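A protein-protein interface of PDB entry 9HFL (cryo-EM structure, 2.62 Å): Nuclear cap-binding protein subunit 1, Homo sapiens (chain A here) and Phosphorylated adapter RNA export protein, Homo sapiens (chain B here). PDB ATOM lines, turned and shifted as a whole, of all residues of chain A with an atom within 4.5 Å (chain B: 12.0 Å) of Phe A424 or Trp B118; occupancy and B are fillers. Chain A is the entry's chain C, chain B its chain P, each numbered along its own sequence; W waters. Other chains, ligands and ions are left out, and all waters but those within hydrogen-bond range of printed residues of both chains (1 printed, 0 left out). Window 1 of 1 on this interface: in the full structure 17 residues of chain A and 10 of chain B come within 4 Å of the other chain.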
ATOM      1  N   ILE A 377      25.283   5.361  -8.154  1.00  0.00           N
ATOM      2  CA  ILE A 377      26.279   5.495  -9.217  1.00  0.00           C
ATOM      3  C   ILE A 377      27.304   4.367  -9.128  1.00  0.00           C
ATOM      4  O   ILE A 377      27.697   3.782 -10.144  1.00  0.00           O
ATOM      5  CB  ILE A 377      26.950   6.878  -9.155  1.00  0.00           C
ATOM      6  CG1 ILE A 377      25.993   7.956  -9.663  1.00  0.00           C
ATOM      7  CG2 ILE A 377      28.225   6.890  -9.979  1.00  0.00           C
ATOM      8  CD1 ILE A 377      26.302   9.335  -9.138  1.00  0.00           C
ATOM      9  N   CYS A 380      25.747   1.173 -10.433  1.00  0.00           N
ATOM     10  CA  CYS A 380      25.691   1.193 -11.891  1.00  0.00           C
ATOM     11  C   CYS A 380      27.062   0.914 -12.492  1.00  0.00           C
ATOM     12  O   CYS A 380      27.175   0.214 -13.502  1.00  0.00           O
ATOM     13  CB  CYS A 380      25.156   2.539 -12.378  1.00  0.00           C
ATOM     14  SG  CYS A 380      23.373   2.740 -12.202  1.00  0.00           S
ATOM     15  N   PRO A 388      21.928  -0.186 -14.699  1.00  0.00           N
ATOM     16  CA  PRO A 388      21.413   1.078 -15.254  1.00  0.00           C
ATOM     17  C   PRO A 388      20.032   0.953 -15.876  1.00  0.00           C
ATOM     18  O   PRO A 388      19.215   1.874 -15.752  1.00  0.00           O
ATOM     19  CB  PRO A 388      22.473   1.454 -16.298  1.00  0.00           C
ATOM     20  CG  PRO A 388      23.705   0.778 -15.854  1.00  0.00           C
ATOM     21  CD  PRO A 388      23.282  -0.492 -15.191  1.00  0.00           C
ATOM     22  N   LEU A 391      17.530   0.821 -13.172  1.00  0.00           N
ATOM     23  CA  LEU A 391      17.389   2.155 -12.602  1.00  0.00           C
ATOM     24  C   LEU A 391      16.520   3.043 -13.481  1.00  0.00           C
ATOM     25  O   LEU A 391      15.700   3.815 -12.976  1.00  0.00           O
ATOM     26  CB  LEU A 391      18.770   2.778 -12.401  1.00  0.00           C
ATOM     27  CG  LEU A 391      18.892   3.987 -11.467  1.00  0.00           C
ATOM     28  CD1 LEU A 391      18.094   3.801 -10.186  1.00  0.00           C
ATOM     29  CD2 LEU A 391      20.356   4.243 -11.149  1.00  0.00           C
ATOM     30  N   ALA A 392      16.689   2.953 -14.801  1.00  0.00           N
ATOM     31  CA  ALA A 392      15.845   3.730 -15.706  1.00  0.00           C
ATOM     32  C   ALA A 392      14.388   3.292 -15.612  1.00  0.00           C
ATOM     33  O   ALA A 392      13.474   4.127 -15.629  1.00  0.00           O
ATOM     34  CB  ALA A 392      16.355   3.599 -17.139  1.00  0.00           C
ATOM     35  N   THR A 395      13.028   4.729 -12.435  1.00  0.00           N
ATOM     36  CA  THR A 395      12.775   6.157 -12.593  1.00  0.00           C
ATOM     37  C   THR A 395      11.481   6.402 -13.353  1.00  0.00           C
ATOM     38  O   THR A 395      10.683   7.270 -12.976  1.00  0.00           O
ATOM     39  CB  THR A 395      13.950   6.818 -13.315  1.00  0.00           C
ATOM     40  OG1 THR A 395      15.170   6.516 -12.627  1.00  0.00           O
ATOM     41  CG2 THR A 395      13.764   8.323 -13.377  1.00  0.00           C
ATOM     42  N   PHE A 417      17.244  12.793  -8.785  1.00  0.00           N
ATOM     43  CA  PHE A 417      17.207  12.652 -10.234  1.00  0.00           C
ATOM     44  C   PHE A 417      18.081  13.697 -10.912  1.00  0.00           C
ATOM     45  O   PHE A 417      18.806  13.382 -11.861  1.00  0.00           O
ATOM     46  CB  PHE A 417      15.764  12.744 -10.730  1.00  0.00           C
ATOM     47  CG  PHE A 417      15.595  12.413 -12.188  1.00  0.00           C
ATOM     48  CD1 PHE A 417      16.305  11.375 -12.770  1.00  0.00           C
ATOM     49  CD2 PHE A 417      14.717  13.135 -12.974  1.00  0.00           C
ATOM     50  CE1 PHE A 417      16.145  11.072 -14.107  1.00  0.00           C
ATOM     51  CE2 PHE A 417      14.554  12.836 -14.311  1.00  0.00           C
ATOM     52  CZ  PHE A 417      15.268  11.803 -14.877  1.00  0.00           C
ATOM     53  N   HIS A 420      21.708  12.767 -10.325  1.00  0.00           N
ATOM     54  CA  HIS A 420      22.059  11.605 -11.131  1.00  0.00           C
ATOM     55  C   HIS A 420      22.253  11.989 -12.591  1.00  0.00           C
ATOM     56  O   HIS A 420      23.222  11.564 -13.229  1.00  0.00           O
ATOM     57  CB  HIS A 420      20.973  10.538 -10.990  1.00  0.00           C
ATOM     58  CG  HIS A 420      21.332   9.222 -11.606  1.00  0.00           C
ATOM     59  ND1 HIS A 420      20.756   8.767 -12.772  1.00  0.00           N
ATOM     60  CD2 HIS A 420      22.207   8.266 -11.219  1.00  0.00           C
ATOM     61  CE1 HIS A 420      21.263   7.588 -13.078  1.00  0.00           C
ATOM     62  NE2 HIS A 420      22.146   7.260 -12.153  1.00  0.00           N
ATOM     63  N   LEU A 421      21.344  12.799 -13.138  1.00  0.00           N
ATOM     64  CA  LEU A 421      21.504  13.263 -14.511  1.00  0.00           C
ATOM     65  C   LEU A 421      22.794  14.053 -14.669  1.00  0.00           C
ATOM     66  O   LEU A 421      23.460  13.966 -15.705  1.00  0.00           O
ATOM     67  CB  LEU A 421      20.303  14.115 -14.920  1.00  0.00           C
ATOM     68  CG  LEU A 421      18.994  13.372 -15.180  1.00  0.00           C
ATOM     69  CD1 LEU A 421      17.893  14.362 -15.492  1.00  0.00           C
ATOM     70  CD2 LEU A 421      19.145  12.368 -16.306  1.00  0.00           C
ATOM     71  N   SER A 422      23.163  14.830 -13.650  1.00  0.00           N
ATOM     72  CA  SER A 422      24.421  15.564 -13.705  1.00  0.00           C
ATOM     73  C   SER A 422      25.614  14.631 -13.876  1.00  0.00           C
ATOM     74  O   SER A 422      26.647  15.039 -14.418  1.00  0.00           O
ATOM     75  CB  SER A 422      24.586  16.405 -12.440  1.00  0.00           C
ATOM     76  OG  SER A 422      25.946  16.515 -12.069  1.00  0.00           O
ATOM     77  N   ASN A 423      25.499  13.387 -13.422  1.00  0.00           N
ATOM     78  CA  ASN A 423      26.586  12.420 -13.501  1.00  0.00           C
ATOM     79  C   ASN A 423      26.522  11.550 -14.749  1.00  0.00           C
ATOM     80  O   ASN A 423      27.433  10.747 -14.970  1.00  0.00           O
ATOM     81  CB  ASN A 423      26.579  11.529 -12.258  1.00  0.00           C
ATOM     82  CG  ASN A 423      27.359  12.128 -11.111  1.00  0.00           C
ATOM     83  OD1 ASN A 423      28.527  11.803 -10.903  1.00  0.00           O
ATOM     84  ND2 ASN A 423      26.718  13.012 -10.359  1.00  0.00           N
ATOM     85  N   PHE A 424      25.481  11.686 -15.564  1.00  0.00           N
ATOM     86  CA  PHE A 424      25.305  10.893 -16.774  1.00  0.00           C
ATOM     87  C   PHE A 424      25.047  11.800 -17.967  1.00  0.00           C
ATOM     88  O   PHE A 424      24.211  11.511 -18.827  1.00  0.00           O
ATOM     89  CB  PHE A 424      24.175   9.880 -16.596  1.00  0.00           C
ATOM     90  CG  PHE A 424      24.545   8.720 -15.719  1.00  0.00           C
ATOM     91  CD1 PHE A 424      24.536   8.847 -14.340  1.00  0.00           C
ATOM     92  CD2 PHE A 424      24.915   7.507 -16.269  1.00  0.00           C
ATOM     93  CE1 PHE A 424      24.885   7.789 -13.530  1.00  0.00           C
ATOM     94  CE2 PHE A 424      25.262   6.443 -15.461  1.00  0.00           C
ATOM     95  CZ  PHE A 424      25.246   6.585 -14.091  1.00  0.00           C
ATOM     96  N   GLN A 425      25.760  12.924 -18.022  1.00  0.00           N
ATOM     97  CA  GLN A 425      25.726  13.838 -19.162  1.00  0.00           C
ATOM     98  C   GLN A 425      24.322  14.369 -19.431  1.00  0.00           C
ATOM     99  O   GLN A 425      23.996  14.738 -20.559  1.00  0.00           O
ATOM    100  CB  GLN A 425      26.287  13.167 -20.418  1.00  0.00           C
ATOM    101  CG  GLN A 425      27.693  12.620 -20.242  1.00  0.00           C
ATOM    102  CD  GLN A 425      28.201  11.904 -21.473  1.00  0.00           C
ATOM    103  OE1 GLN A 425      27.478  11.748 -22.457  1.00  0.00           O
ATOM    104  NE2 GLN A 425      29.448  11.455 -21.423  1.00  0.00           N
ATOM    105  N   PHE A 426      23.483  14.419 -18.397  1.00  0.00           N
ATOM    106  CA  PHE A 426      22.130  14.959 -18.511  1.00  0.00           C
ATOM    107  C   PHE A 426      21.341  14.272 -19.620  1.00  0.00           C
ATOM    108  O   PHE A 426      20.523  14.899 -20.295  1.00  0.00           O
ATOM    109  CB  PHE A 426      22.160  16.472 -18.744  1.00  0.00           C
ATOM    110  CG  PHE A 426      22.733  17.251 -17.596  1.00  0.00           C
ATOM    111  CD1 PHE A 426      21.936  17.620 -16.528  1.00  0.00           C
ATOM    112  CD2 PHE A 426      24.067  17.612 -17.584  1.00  0.00           C
ATOM    113  CE1 PHE A 426      22.459  18.334 -15.472  1.00  0.00           C
ATOM    114  CE2 PHE A 426      24.595  18.327 -16.530  1.00  0.00           C
ATOM    115  CZ  PHE A 426      23.790  18.689 -15.473  1.00  0.00           C
ATOM    116  N   ARG A 427      21.570  12.977 -19.808  1.00  0.00           N
ATOM    117  CA  ARG A 427      20.917  12.218 -20.865  1.00  0.00           C
ATOM    118  C   ARG A 427      19.678  11.537 -20.300  1.00  0.00           C
ATOM    119  O   ARG A 427      19.770  10.772 -19.335  1.00  0.00           O
ATOM    120  CB  ARG A 427      21.873  11.182 -21.455  1.00  0.00           C
ATOM    121  CG  ARG A 427      22.879  11.722 -22.470  1.00  0.00           C
ATOM    122  CD  ARG A 427      22.231  12.551 -23.571  1.00  0.00           C
ATOM    123  NE  ARG A 427      21.153  11.833 -24.241  1.00  0.00           N
ATOM    124  CZ  ARG A 427      21.331  10.807 -25.062  1.00  0.00           C
ATOM    125  NH1 ARG A 427      22.539  10.352 -25.349  1.00  0.00           N
ATOM    126  NH2 ARG A 427      20.269  10.224 -25.610  1.00  0.00           N
ATOM    127  N   TRP A 428      18.524  11.818 -20.898  1.00  0.00           N
ATOM    128  CA  TRP A 428      17.281  11.184 -20.493  1.00  0.00           C
ATOM    129  C   TRP A 428      16.328  11.160 -21.677  1.00  0.00           C
ATOM    130  O   TRP A 428      16.420  11.988 -22.584  1.00  0.00           O
ATOM    131  CB  TRP A 428      16.634  11.908 -19.306  1.00  0.00           C
ATOM    132  CG  TRP A 428      15.385  11.242 -18.837  1.00  0.00           C
ATOM    133  CD1 TRP A 428      14.126  11.761 -18.849  1.00  0.00           C
ATOM    134  CD2 TRP A 428      15.271   9.920 -18.304  1.00  0.00           C
ATOM    135  NE1 TRP A 428      13.234  10.845 -18.353  1.00  0.00           N
ATOM    136  CE2 TRP A 428      13.913   9.706 -18.009  1.00  0.00           C
ATOM    137  CE3 TRP A 428      16.185   8.897 -18.044  1.00  0.00           C
ATOM    138  CZ2 TRP A 428      13.448   8.512 -17.467  1.00  0.00           C
ATOM    139  CZ3 TRP A 428      15.723   7.714 -17.507  1.00  0.00           C
ATOM    140  CH2 TRP A 428      14.367   7.531 -17.224  1.00  0.00           C
ATOM    141  N   LYS B 113      10.048  -2.678 -23.575  1.00  0.00           N
ATOM    142  CA  LYS B 113      11.344  -2.231 -24.059  1.00  0.00           C
ATOM    143  C   LYS B 113      12.275  -1.915 -22.892  1.00  0.00           C
ATOM    144  O   LYS B 113      11.844  -1.646 -21.767  1.00  0.00           O
ATOM    145  CB  LYS B 113      11.190  -1.002 -24.952  1.00  0.00           C
ATOM    146  CG  LYS B 113      11.451  -1.275 -26.425  1.00  0.00           C
ATOM    147  CD  LYS B 113      11.348  -0.008 -27.258  1.00  0.00           C
ATOM    148  CE  LYS B 113      11.619  -0.290 -28.729  1.00  0.00           C
ATOM    149  NZ  LYS B 113      11.390   0.907 -29.586  1.00  0.00           N
ATOM    150  N   ILE B 114      13.574  -1.953 -23.177  1.00  0.00           N
ATOM    151  CA  ILE B 114      14.617  -1.670 -22.200  1.00  0.00           C
ATOM    152  C   ILE B 114      15.163  -0.276 -22.471  1.00  0.00           C
ATOM    153  O   ILE B 114      15.455   0.073 -23.621  1.00  0.00           O
ATOM    154  CB  ILE B 114      15.736  -2.726 -22.261  1.00  0.00           C
ATOM    155  CG1 ILE B 114      15.377  -3.932 -21.393  1.00  0.00           C
ATOM    156  CG2 ILE B 114      17.069  -2.140 -21.815  1.00  0.00           C
ATOM    157  CD1 ILE B 114      14.157  -4.688 -21.870  1.00  0.00           C
ATOM    158  N   ASN B 115      15.296   0.524 -21.415  1.00  0.00           N
ATOM    159  CA  ASN B 115      15.865   1.863 -21.514  1.00  0.00           C
ATOM    160  C   ASN B 115      17.357   1.772 -21.224  1.00  0.00           C
ATOM    161  O   ASN B 115      17.762   1.569 -20.075  1.00  0.00           O
ATOM    162  CB  ASN B 115      15.170   2.814 -20.543  1.00  0.00           C
ATOM    163  CG  ASN B 115      14.987   4.205 -21.115  1.00  0.00           C
ATOM    164  OD1 ASN B 115      15.584   4.556 -22.130  1.00  0.00           O
ATOM    165  ND2 ASN B 115      14.158   5.006 -20.461  1.00  0.00           N
ATOM    166  N   ASN B 116      18.177   1.923 -22.264  1.00  0.00           N
ATOM    167  CA  ASN B 116      19.623   1.789 -22.153  1.00  0.00           C
ATOM    168  C   ASN B 116      20.344   3.126 -22.286  1.00  0.00           C
ATOM    169  O   ASN B 116      21.548   3.150 -22.566  1.00  0.00           O
ATOM    170  CB  ASN B 116      20.137   0.806 -23.205  1.00  0.00           C
ATOM    171  CG  ASN B 116      21.484   0.217 -22.843  1.00  0.00           C
ATOM    172  OD1 ASN B 116      21.625  -0.460 -21.828  1.00  0.00           O
ATOM    173  ND2 ASN B 116      22.485   0.470 -23.679  1.00  0.00           N
ATOM    174  N   ILE B 117      19.638   4.240 -22.087  1.00  0.00           N
ATOM    175  CA  ILE B 117      20.265   5.552 -22.235  1.00  0.00           C
ATOM    176  C   ILE B 117      21.435   5.692 -21.268  1.00  0.00           C
ATOM    177  O   ILE B 117      22.550   6.068 -21.657  1.00  0.00           O
ATOM    178  CB  ILE B 117      19.223   6.668 -22.037  1.00  0.00           C
ATOM    179  CG1 ILE B 117      19.858   8.041 -22.263  1.00  0.00           C
ATOM    180  CG2 ILE B 117      18.590   6.599 -20.648  1.00  0.00           C
ATOM    181  CD1 ILE B 117      18.965   9.001 -23.005  1.00  0.00           C
ATOM    182  N   TRP B 118      21.209   5.367 -19.994  1.00  0.00           N
ATOM    183  CA  TRP B 118      22.283   5.468 -19.015  1.00  0.00           C
ATOM    184  C   TRP B 118      23.329   4.385 -19.222  1.00  0.00           C
ATOM    185  O   TRP B 118      24.507   4.612 -18.942  1.00  0.00           O
ATOM    186  CB  TRP B 118      21.713   5.406 -17.598  1.00  0.00           C
ATOM    187  CG  TRP B 118      20.877   6.598 -17.248  1.00  0.00           C
ATOM    188  CD1 TRP B 118      20.936   7.837 -17.818  1.00  0.00           C
ATOM    189  CD2 TRP B 118      19.851   6.663 -16.253  1.00  0.00           C
ATOM    190  NE1 TRP B 118      20.011   8.667 -17.241  1.00  0.00           N
ATOM    191  CE2 TRP B 118      19.332   7.971 -16.276  1.00  0.00           C
ATOM    192  CE3 TRP B 118      19.320   5.743 -15.346  1.00  0.00           C
ATOM    193  CZ2 TRP B 118      18.311   8.382 -15.425  1.00  0.00           C
ATOM    194  CZ3 TRP B 118      18.307   6.152 -14.505  1.00  0.00           C
ATOM    195  CH2 TRP B 118      17.813   7.460 -14.549  1.00  0.00           C
ATOM    196  N   GLY B 119      22.930   3.215 -19.720  1.00  0.00           N
ATOM    197  CA  GLY B 119      23.915   2.204 -20.065  1.00  0.00           C
ATOM    198  C   GLY B 119      24.843   2.659 -21.175  1.00  0.00           C
ATOM    199  O   GLY B 119      26.058   2.455 -21.107  1.00  0.00           O
ATOM    200  N   ALA B 120      24.284   3.288 -22.212  1.00  0.00           N
ATOM    201  CA  ALA B 120      25.112   3.833 -23.280  1.00  0.00           C
ATOM    202  C   ALA B 120      26.025   4.936 -22.760  1.00  0.00           C
ATOM    203  O   ALA B 120      27.209   4.996 -23.119  1.00  0.00           O
ATOM    204  CB  ALA B 120      24.227   4.358 -24.408  1.00  0.00           C
ATOM    205  N   VAL B 121      25.493   5.818 -21.909  1.00  0.00           N
ATOM    206  CA  VAL B 121      26.323   6.878 -21.341  1.00  0.00           C
ATOM    207  C   VAL B 121      27.462   6.280 -20.526  1.00  0.00           C
ATOM    208  O   VAL B 121      28.600   6.759 -20.578  1.00  0.00           O
ATOM    209  CB  VAL B 121      25.465   7.832 -20.490  1.00  0.00           C
ATOM    210  CG1 VAL B 121      26.354   8.758 -19.679  1.00  0.00           C
ATOM    211  CG2 VAL B 121      24.526   8.630 -21.373  1.00  0.00           C
ATOM    212  N   LEU B 122      27.172   5.237 -19.749  1.00  0.00           N
ATOM    213  CA  LEU B 122      28.197   4.618 -18.920  1.00  0.00           C
ATOM    214  C   LEU B 122      29.249   3.921 -19.772  1.00  0.00           C
ATOM    215  O   LEU B 122      30.436   3.931 -19.432  1.00  0.00           O
ATOM    216  CB  LEU B 122      27.547   3.638 -17.944  1.00  0.00           C
ATOM    217  CG  LEU B 122      28.468   2.929 -16.953  1.00  0.00           C
ATOM    218  CD1 LEU B 122      29.285   3.927 -16.152  1.00  0.00           C
ATOM    219  CD2 LEU B 122      27.647   2.052 -16.029  1.00  0.00           C
ATOM    220  N   GLN B 123      28.834   3.307 -20.882  1.00  0.00           N
ATOM    221  CA  GLN B 123      29.804   2.727 -21.804  1.00  0.00           C
ATOM    222  C   GLN B 123      30.711   3.802 -22.389  1.00  0.00           C
ATOM    223  O   GLN B 123      31.930   3.612 -22.495  1.00  0.00           O
ATOM    224  CB  GLN B 123      29.078   1.969 -22.916  1.00  0.00           C
ATOM    225  CG  GLN B 123      29.998   1.271 -23.912  1.00  0.00           C
ATOM    226  CD  GLN B 123      30.979   0.318 -23.250  1.00  0.00           C
ATOM    227  OE1 GLN B 123      32.167   0.313 -23.571  1.00  0.00           O
ATOM    228  NE2 GLN B 123      30.485  -0.494 -22.324  1.00  0.00           N
ATOM    229  N   GLU B 124      30.135   4.945 -22.768  1.00  0.00           N
ATOM    230  CA  GLU B 124      30.948   6.045 -23.281  1.00  0.00           C
ATOM    231  C   GLU B 124      31.920   6.553 -22.223  1.00  0.00           C
ATOM    232  O   GLU B 124      33.081   6.851 -22.526  1.00  0.00           O
ATOM    233  CB  GLU B 124      30.048   7.178 -23.766  1.00  0.00           C
ATOM    234  CG  GLU B 124      29.339   6.883 -25.074  1.00  0.00           C
ATOM    235  CD  GLU B 124      28.214   7.855 -25.365  1.00  0.00           C
ATOM    236  OE1 GLU B 124      27.774   8.560 -24.432  1.00  0.00           O
ATOM    237  OE2 GLU B 124      27.770   7.916 -26.530  1.00  0.00           O
ATOM    238  N   GLN B 125      31.462   6.666 -20.976  1.00  0.00           N
ATOM    239  CA  GLN B 125      32.340   7.118 -19.902  1.00  0.00           C
ATOM    240  C   GLN B 125      33.458   6.118 -19.644  1.00  0.00           C
ATOM    241  O   GLN B 125      34.594   6.510 -19.361  1.00  0.00           O
ATOM    242  CB  GLN B 125      31.530   7.362 -18.630  1.00  0.00           C
ATOM    243  CG  GLN B 125      30.645   8.593 -18.698  1.00  0.00           C
ATOM    244  CD  GLN B 125      29.783   8.761 -17.468  1.00  0.00           C
ATOM    245  OE1 GLN B 125      29.565   7.814 -16.714  1.00  0.00           O
ATOM    246  NE2 GLN B 125      29.281   9.971 -17.259  1.00  0.00           N
ATOM    247  N   ASN B 126      33.154   4.821 -19.721  1.00  0.00           N
ATOM    248  CA  ASN B 126      34.194   3.807 -19.575  1.00  0.00           C
ATOM    249  C   ASN B 126      35.216   3.911 -20.698  1.00  0.00           C
ATOM    250  O   ASN B 126      36.423   3.765 -20.470  1.00  0.00           O
ATOM    251  CB  ASN B 126      33.565   2.415 -19.548  1.00  0.00           C
ATOM    252  CG  ASN B 126      34.440   1.394 -18.850  1.00  0.00           C
ATOM    253  OD1 ASN B 126      35.245   1.736 -17.985  1.00  0.00           O
ATOM    254  ND2 ASN B 126      34.286   0.131 -19.227  1.00  0.00           N
ATOM    255  N   GLN B 127      34.749   4.158 -21.924  1.00  0.00           N
ATOM    256  CA  GLN B 127      35.671   4.369 -23.034  1.00  0.00           C
ATOM    257  C   GLN B 127      36.561   5.581 -22.786  1.00  0.00           C
ATOM    258  O   GLN B 127      37.770   5.538 -23.042  1.00  0.00           O
ATOM    259  CB  GLN B 127      34.887   4.541 -24.334  1.00  0.00           C
ATOM    260  CG  GLN B 127      35.569   3.948 -25.549  1.00  0.00           C
ATOM    261  CD  GLN B 127      34.685   3.975 -26.776  1.00  0.00           C
ATOM    262  OE1 GLN B 127      33.459   3.994 -26.670  1.00  0.00           O
ATOM    263  NE2 GLN B 127      35.304   3.972 -27.951  1.00  0.00           N
ATOM    264  N   ASP B 128      35.978   6.676 -22.291  1.00  0.00           N
ATOM    265  CA  ASP B 128      36.767   7.866 -21.988  1.00  0.00           C
ATOM    266  C   ASP B 128      37.794   7.583 -20.898  1.00  0.00           C
ATOM    267  O   ASP B 128      38.931   8.061 -20.965  1.00  0.00           O
ATOM    268  CB  ASP B 128      35.851   9.012 -21.563  1.00  0.00           C
ATOM    269  CG  ASP B 128      34.964   9.501 -22.688  1.00  0.00           C
ATOM    270  OD1 ASP B 128      35.255   9.182 -23.859  1.00  0.00           O
ATOM    271  OD2 ASP B 128      33.976  10.207 -22.400  1.00  0.00           O
HETATM  272  O   HOH W   1      19.574   2.621 -18.766  1.00  0.00           O
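The backbone carbonyl oxygen (O) of Asn A423 lies within hydrogen-bond range of the side-chain amide nitrogen (NE2) of Gln B125 (3.0 Å). The indole nitrogen of Trp B118 lies within hydrogen-bond range of the backbone carbonyl oxygen of Arg A427.
The backbone carbonyl oxygen (O) of Leu A391 lies within hydrogen-bond range of the side-chain hydroxyl (OG1) of Thr A395, 2.8 Å away. The backbone carbonyl oxygen (O) of Leu A421 sits at hydrogen-bond distance from the backbone NH (N) of Phe A426, at 2.7 Å.
Among the printed residues, pairs that only touch across the chains: Arg A427 with Ile B117, Cys A380 with Leu B122, Trp A428 with Trp B118, Thr A395 with Trp B118, His A420 with Trp B118, Trp A428 with Ile B117, Phe A424 with Val B121, Ala A392 with Trp B118, Arg A427 with Val B121, Ala A392 with Asn B115, Phe A417 with Trp B118, Leu A391 with Trp B118, Gln A425 with Glu B124, Pro A388 with Gly B119, Pro A388 with Trp B118, Leu A421 with Trp B118 and Phe A424 with Trp B118.
Phe A424 touches just these residues of chain B: Trp B118 and Val B121. Pro A388 touches just these residues of chain B: Trp B118 and Gly B119. Of chain B, only Trp B118 (3.7 Å) comes within 4 Å of Leu A391. Of the printed residues of chain B, Ala A392 touches Asn B115 (3.7 Å) and Trp B118 (3.6 Å). Of chain B, only Trp B118 comes within 4 Å of Thr A395. His A420 touches one residue of chain B. Of the printed residues of chain B, Gln A425 touches Glu B124. No residue of chain B comes within 4 Å of Phe A426. Arg A427 touches just these residues of chain B: Ile B117, Trp B118 and Val B121. Trp A428 touches two residues of chain B. Printed residues of chain A within 4 Å of Gly B119: Pro A388. Of the printed residues of chain A, Ile B117 touches Arg A427 and Trp A428. Gln B127 touches none of the printed residues of chain A. Asn B126 touches none of the printed residues of chain A. The nearest residue of chain B that does not touch Phe A424 is Gln B125 (4.1 Å). The nearest printed residue of chain A that does not touch Trp B118 is Cys A380 (5.9 Å). The nearest printed residue of chain A that does not touch Asn B115 is Trp A428 (4.1 Å).
Hydrophobic or aromatic side chains of chain A within 4 Å of the printed part of chain B: Pro A388, Leu A391, Ala A392, Phe A417, His A420, Leu A421, Phe A424 and Trp A428. Among the printed residues, 19 pairs touch across the chains. Among the printed residues, no Asp or Glu carboxylate lies within 4 Å of a Lys or Arg side-chain nitrogen of the other chain.
Water W1 lies within hydrogen-bond range of the backbone carbonyl oxygen of Asn B115, the backbone carbonyl oxygen of Pro A388 and the backbone NH of Trp B118.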
